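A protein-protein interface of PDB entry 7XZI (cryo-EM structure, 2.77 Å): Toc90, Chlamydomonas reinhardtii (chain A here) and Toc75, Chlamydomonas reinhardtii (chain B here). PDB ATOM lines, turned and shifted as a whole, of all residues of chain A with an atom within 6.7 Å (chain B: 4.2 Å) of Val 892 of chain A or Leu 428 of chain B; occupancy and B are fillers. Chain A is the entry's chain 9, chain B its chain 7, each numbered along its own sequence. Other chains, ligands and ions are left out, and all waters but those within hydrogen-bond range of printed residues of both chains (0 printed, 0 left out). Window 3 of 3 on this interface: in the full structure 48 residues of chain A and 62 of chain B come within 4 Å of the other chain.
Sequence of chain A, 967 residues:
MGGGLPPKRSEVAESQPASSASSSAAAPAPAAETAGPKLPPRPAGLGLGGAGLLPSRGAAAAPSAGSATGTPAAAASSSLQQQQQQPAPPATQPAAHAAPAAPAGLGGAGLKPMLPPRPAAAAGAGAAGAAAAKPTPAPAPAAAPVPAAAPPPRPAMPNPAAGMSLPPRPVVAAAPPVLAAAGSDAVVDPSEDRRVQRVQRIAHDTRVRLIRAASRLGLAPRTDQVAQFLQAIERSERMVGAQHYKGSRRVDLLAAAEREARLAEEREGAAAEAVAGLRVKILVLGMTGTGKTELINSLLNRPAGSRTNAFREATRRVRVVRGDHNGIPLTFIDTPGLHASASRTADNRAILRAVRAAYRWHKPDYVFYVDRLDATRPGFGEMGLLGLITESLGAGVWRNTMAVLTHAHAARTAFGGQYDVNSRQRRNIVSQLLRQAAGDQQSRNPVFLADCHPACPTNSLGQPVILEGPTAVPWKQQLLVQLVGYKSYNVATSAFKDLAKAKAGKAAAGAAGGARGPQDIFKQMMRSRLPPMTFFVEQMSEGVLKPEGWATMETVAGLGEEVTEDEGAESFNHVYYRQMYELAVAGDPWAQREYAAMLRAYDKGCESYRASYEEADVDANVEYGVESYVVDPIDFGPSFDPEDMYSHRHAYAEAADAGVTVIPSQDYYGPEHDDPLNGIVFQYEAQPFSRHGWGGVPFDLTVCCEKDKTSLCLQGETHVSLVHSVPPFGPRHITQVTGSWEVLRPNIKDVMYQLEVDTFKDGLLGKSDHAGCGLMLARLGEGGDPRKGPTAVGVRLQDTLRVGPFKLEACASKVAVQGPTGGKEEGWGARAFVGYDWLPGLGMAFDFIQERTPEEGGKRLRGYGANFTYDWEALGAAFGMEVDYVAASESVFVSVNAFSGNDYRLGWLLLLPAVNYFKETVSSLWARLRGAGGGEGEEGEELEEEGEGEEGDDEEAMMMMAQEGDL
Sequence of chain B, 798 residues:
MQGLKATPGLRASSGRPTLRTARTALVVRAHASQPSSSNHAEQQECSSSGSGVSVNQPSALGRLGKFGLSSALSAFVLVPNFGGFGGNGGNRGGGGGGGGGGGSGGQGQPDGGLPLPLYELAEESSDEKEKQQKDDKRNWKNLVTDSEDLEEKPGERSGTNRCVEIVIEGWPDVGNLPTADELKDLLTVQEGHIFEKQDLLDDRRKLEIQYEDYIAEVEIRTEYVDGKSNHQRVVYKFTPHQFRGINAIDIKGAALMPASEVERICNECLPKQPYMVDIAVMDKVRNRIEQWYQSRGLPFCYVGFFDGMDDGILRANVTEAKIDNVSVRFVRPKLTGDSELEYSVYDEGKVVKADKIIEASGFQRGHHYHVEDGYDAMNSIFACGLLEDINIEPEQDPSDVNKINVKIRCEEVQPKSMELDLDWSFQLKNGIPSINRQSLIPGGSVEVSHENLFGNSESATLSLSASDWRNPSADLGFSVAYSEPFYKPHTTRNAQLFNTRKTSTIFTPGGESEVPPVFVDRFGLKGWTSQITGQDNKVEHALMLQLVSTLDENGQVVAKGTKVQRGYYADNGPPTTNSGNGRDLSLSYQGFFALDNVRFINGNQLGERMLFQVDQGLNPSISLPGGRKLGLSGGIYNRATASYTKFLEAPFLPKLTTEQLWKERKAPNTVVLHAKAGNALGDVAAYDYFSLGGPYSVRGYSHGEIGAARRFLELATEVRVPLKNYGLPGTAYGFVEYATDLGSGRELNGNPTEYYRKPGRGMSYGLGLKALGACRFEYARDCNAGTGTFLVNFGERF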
ATOM      1  N   VAL A 883       3.155   9.677  30.738  1.00  0.00           N
ATOM      2  CA  VAL A 883       3.826   9.786  29.449  1.00  0.00           C
ATOM      3  C   VAL A 883       4.647  11.068  29.445  1.00  0.00           C
ATOM      4  O   VAL A 883       4.118  12.152  29.719  1.00  0.00           O
ATOM      5  CB  VAL A 883       2.821   9.776  28.281  1.00  0.00           C
ATOM      6  CG1 VAL A 883       3.548   9.923  26.953  1.00  0.00           C
ATOM      7  CG2 VAL A 883       1.995   8.499  28.304  1.00  0.00           C
ATOM      8  N   ASP A 884       5.934  10.944  29.133  1.00  0.00           N
ATOM      9  CA  ASP A 884       6.847  12.079  29.069  1.00  0.00           C
ATOM     10  C   ASP A 884       7.442  12.147  27.670  1.00  0.00           C
ATOM     11  O   ASP A 884       8.039  11.173  27.200  1.00  0.00           O
ATOM     12  CB  ASP A 884       7.952  11.958  30.121  1.00  0.00           C
ATOM     13  N   TYR A 885       7.285  13.292  27.013  1.00  0.00           N
ATOM     14  CA  TYR A 885       7.751  13.493  25.649  1.00  0.00           C
ATOM     15  C   TYR A 885       8.728  14.659  25.613  1.00  0.00           C
ATOM     16  O   TYR A 885       8.418  15.751  26.106  1.00  0.00           O
ATOM     17  CB  TYR A 885       6.571  13.745  24.706  1.00  0.00           C
ATOM     18  CG  TYR A 885       6.907  14.572  23.486  1.00  0.00           C
ATOM     19  CD1 TYR A 885       7.630  14.032  22.433  1.00  0.00           C
ATOM     20  CD2 TYR A 885       6.487  15.892  23.385  1.00  0.00           C
ATOM     21  CE1 TYR A 885       7.935  14.786  21.315  1.00  0.00           C
ATOM     22  CE2 TYR A 885       6.786  16.653  22.273  1.00  0.00           C
ATOM     23  CZ  TYR A 885       7.510  16.095  21.241  1.00  0.00           C
ATOM     24  OH  TYR A 885       7.809  16.851  20.130  1.00  0.00           O
ATOM     25  N   VAL A 886       9.902  14.424  25.032  1.00  0.00           N
ATOM     26  CA  VAL A 886      10.928  15.445  24.868  1.00  0.00           C
ATOM     27  C   VAL A 886      11.260  15.555  23.386  1.00  0.00           C
ATOM     28  O   VAL A 886      11.542  14.544  22.729  1.00  0.00           O
ATOM     29  CB  VAL A 886      12.186  15.131  25.701  1.00  0.00           C
ATOM     30  CG1 VAL A 886      12.577  13.668  25.562  1.00  0.00           C
ATOM     31  CG2 VAL A 886      13.337  16.041  25.295  1.00  0.00           C
ATOM     32  N   GLU A 890      13.910  13.789  20.910  1.00  0.00           N
ATOM     33  CA  GLU A 890      12.868  13.034  20.215  1.00  0.00           C
ATOM     34  C   GLU A 890      12.623  11.690  20.902  1.00  0.00           C
ATOM     35  O   GLU A 890      12.775  10.618  20.313  1.00  0.00           O
ATOM     36  CB  GLU A 890      13.226  12.843  18.738  1.00  0.00           C
ATOM     37  CG  GLU A 890      13.316  14.133  17.940  1.00  0.00           C
ATOM     38  CD  GLU A 890      11.958  14.652  17.511  1.00  0.00           C
ATOM     39  OE1 GLU A 890      11.007  13.845  17.439  1.00  0.00           O
ATOM     40  OE2 GLU A 890      11.841  15.866  17.244  1.00  0.00           O
ATOM     41  N   SER A 891      12.234  11.764  22.173  1.00  0.00           N
ATOM     42  CA  SER A 891      12.073  10.577  23.001  1.00  0.00           C
ATOM     43  C   SER A 891      10.734  10.610  23.723  1.00  0.00           C
ATOM     44  O   SER A 891      10.242  11.678  24.101  1.00  0.00           O
ATOM     45  CB  SER A 891      13.211  10.452  24.022  1.00  0.00           C
ATOM     46  OG  SER A 891      14.467  10.337  23.376  1.00  0.00           O
ATOM     47  N   VAL A 892      10.146   9.428  23.898  1.00  0.00           N
ATOM     48  CA  VAL A 892       8.890   9.255  24.618  1.00  0.00           C
ATOM     49  C   VAL A 892       9.066   8.122  25.620  1.00  0.00           C
ATOM     50  O   VAL A 892       9.496   7.023  25.251  1.00  0.00           O
ATOM     51  CB  VAL A 892       7.718   8.961  23.664  1.00  0.00           C
ATOM     52  CG1 VAL A 892       6.494   8.504  24.445  1.00  0.00           C
ATOM     53  CG2 VAL A 892       7.391  10.192  22.834  1.00  0.00           C
ATOM     54  N   PHE A 893       8.736   8.389  26.881  1.00  0.00           N
ATOM     55  CA  PHE A 893       8.822   7.405  27.953  1.00  0.00           C
ATOM     56  C   PHE A 893       7.444   7.209  28.564  1.00  0.00           C
ATOM     57  O   PHE A 893       6.789   8.182  28.953  1.00  0.00           O
ATOM     58  CB  PHE A 893       9.820   7.842  29.029  1.00  0.00           C
ATOM     59  CG  PHE A 893      11.235   7.952  28.535  1.00  0.00           C
ATOM     60  CD1 PHE A 893      12.086   6.861  28.588  1.00  0.00           C
ATOM     61  CD2 PHE A 893      11.713   9.145  28.022  1.00  0.00           C
ATOM     62  CE1 PHE A 893      13.388   6.958  28.136  1.00  0.00           C
ATOM     63  CE2 PHE A 893      13.014   9.250  27.568  1.00  0.00           C
ATOM     64  CZ  PHE A 893      13.853   8.154  27.625  1.00  0.00           C
ATOM     65  N   VAL A 894       7.012   5.955  28.656  1.00  0.00           N
ATOM     66  CA  VAL A 894       5.706   5.602  29.199  1.00  0.00           C
ATOM     67  C   VAL A 894       5.918   4.694  30.402  1.00  0.00           C
ATOM     68  O   VAL A 894       6.614   3.677  30.303  1.00  0.00           O
ATOM     69  CB  VAL A 894       4.820   4.912  28.146  1.00  0.00           C
ATOM     70  CG1 VAL A 894       3.471   4.547  28.745  1.00  0.00           C
ATOM     71  CG2 VAL A 894       4.648   5.809  26.929  1.00  0.00           C
ATOM     72  N   SER B 425      10.040   2.555  26.489  1.00  0.00           N
ATOM     73  CA  SER B 425      10.812   3.578  25.800  1.00  0.00           C
ATOM     74  C   SER B 425      10.657   3.387  24.299  1.00  0.00           C
ATOM     75  O   SER B 425      10.797   2.271  23.791  1.00  0.00           O
ATOM     76  CB  SER B 425      12.294   3.524  26.194  1.00  0.00           C
ATOM     77  OG  SER B 425      13.023   4.569  25.572  1.00  0.00           O
ATOM     78  N   PHE B 426      10.365   4.477  23.594  1.00  0.00           N
ATOM     79  CA  PHE B 426      10.104   4.435  22.161  1.00  0.00           C
ATOM     80  C   PHE B 426      10.992   5.439  21.443  1.00  0.00           C
ATOM     81  O   PHE B 426      11.077   6.602  21.852  1.00  0.00           O
ATOM     82  CB  PHE B 426       8.630   4.728  21.858  1.00  0.00           C
ATOM     83  CG  PHE B 426       7.698   3.619  22.252  1.00  0.00           C
ATOM     84  CD1 PHE B 426       7.216   3.526  23.548  1.00  0.00           C
ATOM     85  CD2 PHE B 426       7.303   2.670  21.325  1.00  0.00           C
ATOM     86  CE1 PHE B 426       6.358   2.505  23.909  1.00  0.00           C
ATOM     87  CE2 PHE B 426       6.445   1.648  21.681  1.00  0.00           C
ATOM     88  CZ  PHE B 426       5.972   1.566  22.975  1.00  0.00           C
ATOM     89  N   GLN B 427      11.647   4.989  20.375  1.00  0.00           N
ATOM     90  CA  GLN B 427      12.428   5.870  19.508  1.00  0.00           C
ATOM     91  C   GLN B 427      11.499   6.370  18.408  1.00  0.00           C
ATOM     92  O   GLN B 427      11.295   5.696  17.397  1.00  0.00           O
ATOM     93  CB  GLN B 427      13.637   5.138  18.938  1.00  0.00           C
ATOM     94  N   LEU B 428      10.932   7.560  18.613  1.00  0.00           N
ATOM     95  CA  LEU B 428       9.923   8.072  17.691  1.00  0.00           C
ATOM     96  C   LEU B 428      10.515   8.383  16.322  1.00  0.00           C
ATOM     97  O   LEU B 428       9.890   8.096  15.293  1.00  0.00           O
ATOM     98  CB  LEU B 428       9.258   9.316  18.280  1.00  0.00           C
ATOM     99  CG  LEU B 428       7.914   9.116  18.983  1.00  0.00           C
ATOM    100  CD1 LEU B 428       6.820   8.849  17.964  1.00  0.00           C
ATOM    101  CD2 LEU B 428       7.991   7.981  19.994  1.00  0.00           C
ATOM    102  N   LYS B 429      11.717   8.963  16.290  1.00  0.00           N
ATOM    103  CA  LYS B 429      12.357   9.431  15.056  1.00  0.00           C
ATOM    104  C   LYS B 429      11.399  10.421  14.403  1.00  0.00           C
ATOM    105  O   LYS B 429      11.118  11.469  15.011  1.00  0.00           O
ATOM    106  CB  LYS B 429      12.767   8.230  14.201  1.00  0.00           C
ATOM    107  N   ASN B 430      10.879  10.156  13.209  1.00  0.00           N
ATOM    108  CA  ASN B 430       9.887  11.010  12.573  1.00  0.00           C
ATOM    109  C   ASN B 430       8.607  10.220  12.332  1.00  0.00           C
ATOM    110  O   ASN B 430       8.650   9.080  11.857  1.00  0.00           O
ATOM    111  CB  ASN B 430      10.411  11.577  11.249  1.00  0.00           C
ATOM    112  CG  ASN B 430       9.465  12.593  10.635  1.00  0.00           C
ATOM    113  OD1 ASN B 430       9.535  13.784  10.938  1.00  0.00           O
ATOM    114  ND2 ASN B 430       8.576  12.126   9.768  1.00  0.00           N
ATOM    115  N   GLY B 431       7.472  10.832  12.661  1.00  0.00           N
ATOM    116  CA  GLY B 431       6.194  10.171  12.473  1.00  0.00           C
ATOM    117  C   GLY B 431       5.908   9.140  13.554  1.00  0.00           C
ATOM    118  O   GLY B 431       6.425   9.207  14.670  1.00  0.00           O
ATOM    119  N   ILE B 432       5.063   8.173  13.205  1.00  0.00           N
ATOM    120  CA  ILE B 432       4.648   7.118  14.126  1.00  0.00           C
ATOM    121  C   ILE B 432       5.846   6.240  14.468  1.00  0.00           C
ATOM    122  O   ILE B 432       6.727   6.038  13.620  1.00  0.00           O
ATOM    123  CB  ILE B 432       3.504   6.281  13.529  1.00  0.00           C
ATOM    124  N   PRO B 433       5.923   5.703  15.681  1.00  0.00           N
ATOM    125  CA  PRO B 433       7.058   4.852  16.050  1.00  0.00           C
ATOM    126  C   PRO B 433       6.892   3.436  15.512  1.00  0.00           C
ATOM    127  O   PRO B 433       5.871   3.071  14.928  1.00  0.00           O
ATOM    128  CB  PRO B 433       7.022   4.870  17.580  1.00  0.00           C
ATOM    129  CG  PRO B 433       5.574   5.033  17.898  1.00  0.00           C
ATOM    130  CD  PRO B 433       5.000   5.909  16.811  1.00  0.00           C
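N of Phe 426 of chain B lies within hydrogen-bond range of O of Val 892 of chain A.
The side-chain carboxylate (OE1) of Glu 890 of chain A sits close to the backbone carbonyl oxygen (O) of Lys 429 of chain B (3.4 Å).
The backbone carbonyl oxygen of Asp 884 of chain A lies within hydrogen-bond range of the backbone NH of Phe 893 of chain A (2.9 Å).
Among the printed residues, pairs that only touch across the chains: Glu 890 of chain A with Leu 428 of chain B (3.95 Å), Val 892 of chain A with Ser 425 of chain B (3.7 Å), Val 892 of chain A with Leu 428 of chain B (3.6 Å) and Phe 893 of chain A with Ser 425 of chain B (3.5 Å).
Of the printed residues of chain B, Glu 890 of chain A touches Leu 428 and Lys 429.
Val 892 of chain A touches just these residues of chain B: Ser 425 (3.7 Å), Phe 426 (3.2 Å) and Leu 428 (3.6 Å).
Printed residues of chain B within 4 Å of Phe 893 of chain A: Ser 425.
Of the printed residues of chain A, Ser 425 of chain B touches Val 892 (3.7 Å) and Phe 893 (3.5 Å).
Printed residues of chain A within 4 Å of Lys 429 of chain B: Glu 890.
The nearest printed residue of chain A that does not touch Phe 426 of chain B is Ser 891 of chain A (4.3 Å).
Printed residues of chain A that touch a printed residue of chain B: Glu 890, Val 892 and Phe 893.
Hydrophobic or aromatic side chains of chain A that line the printed part of chain B: Val 892 and Phe 893.
Printed residues of chain B that touch a printed residue of chain A: Ser 425, Phe 426, Leu 428 and Lys 429.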
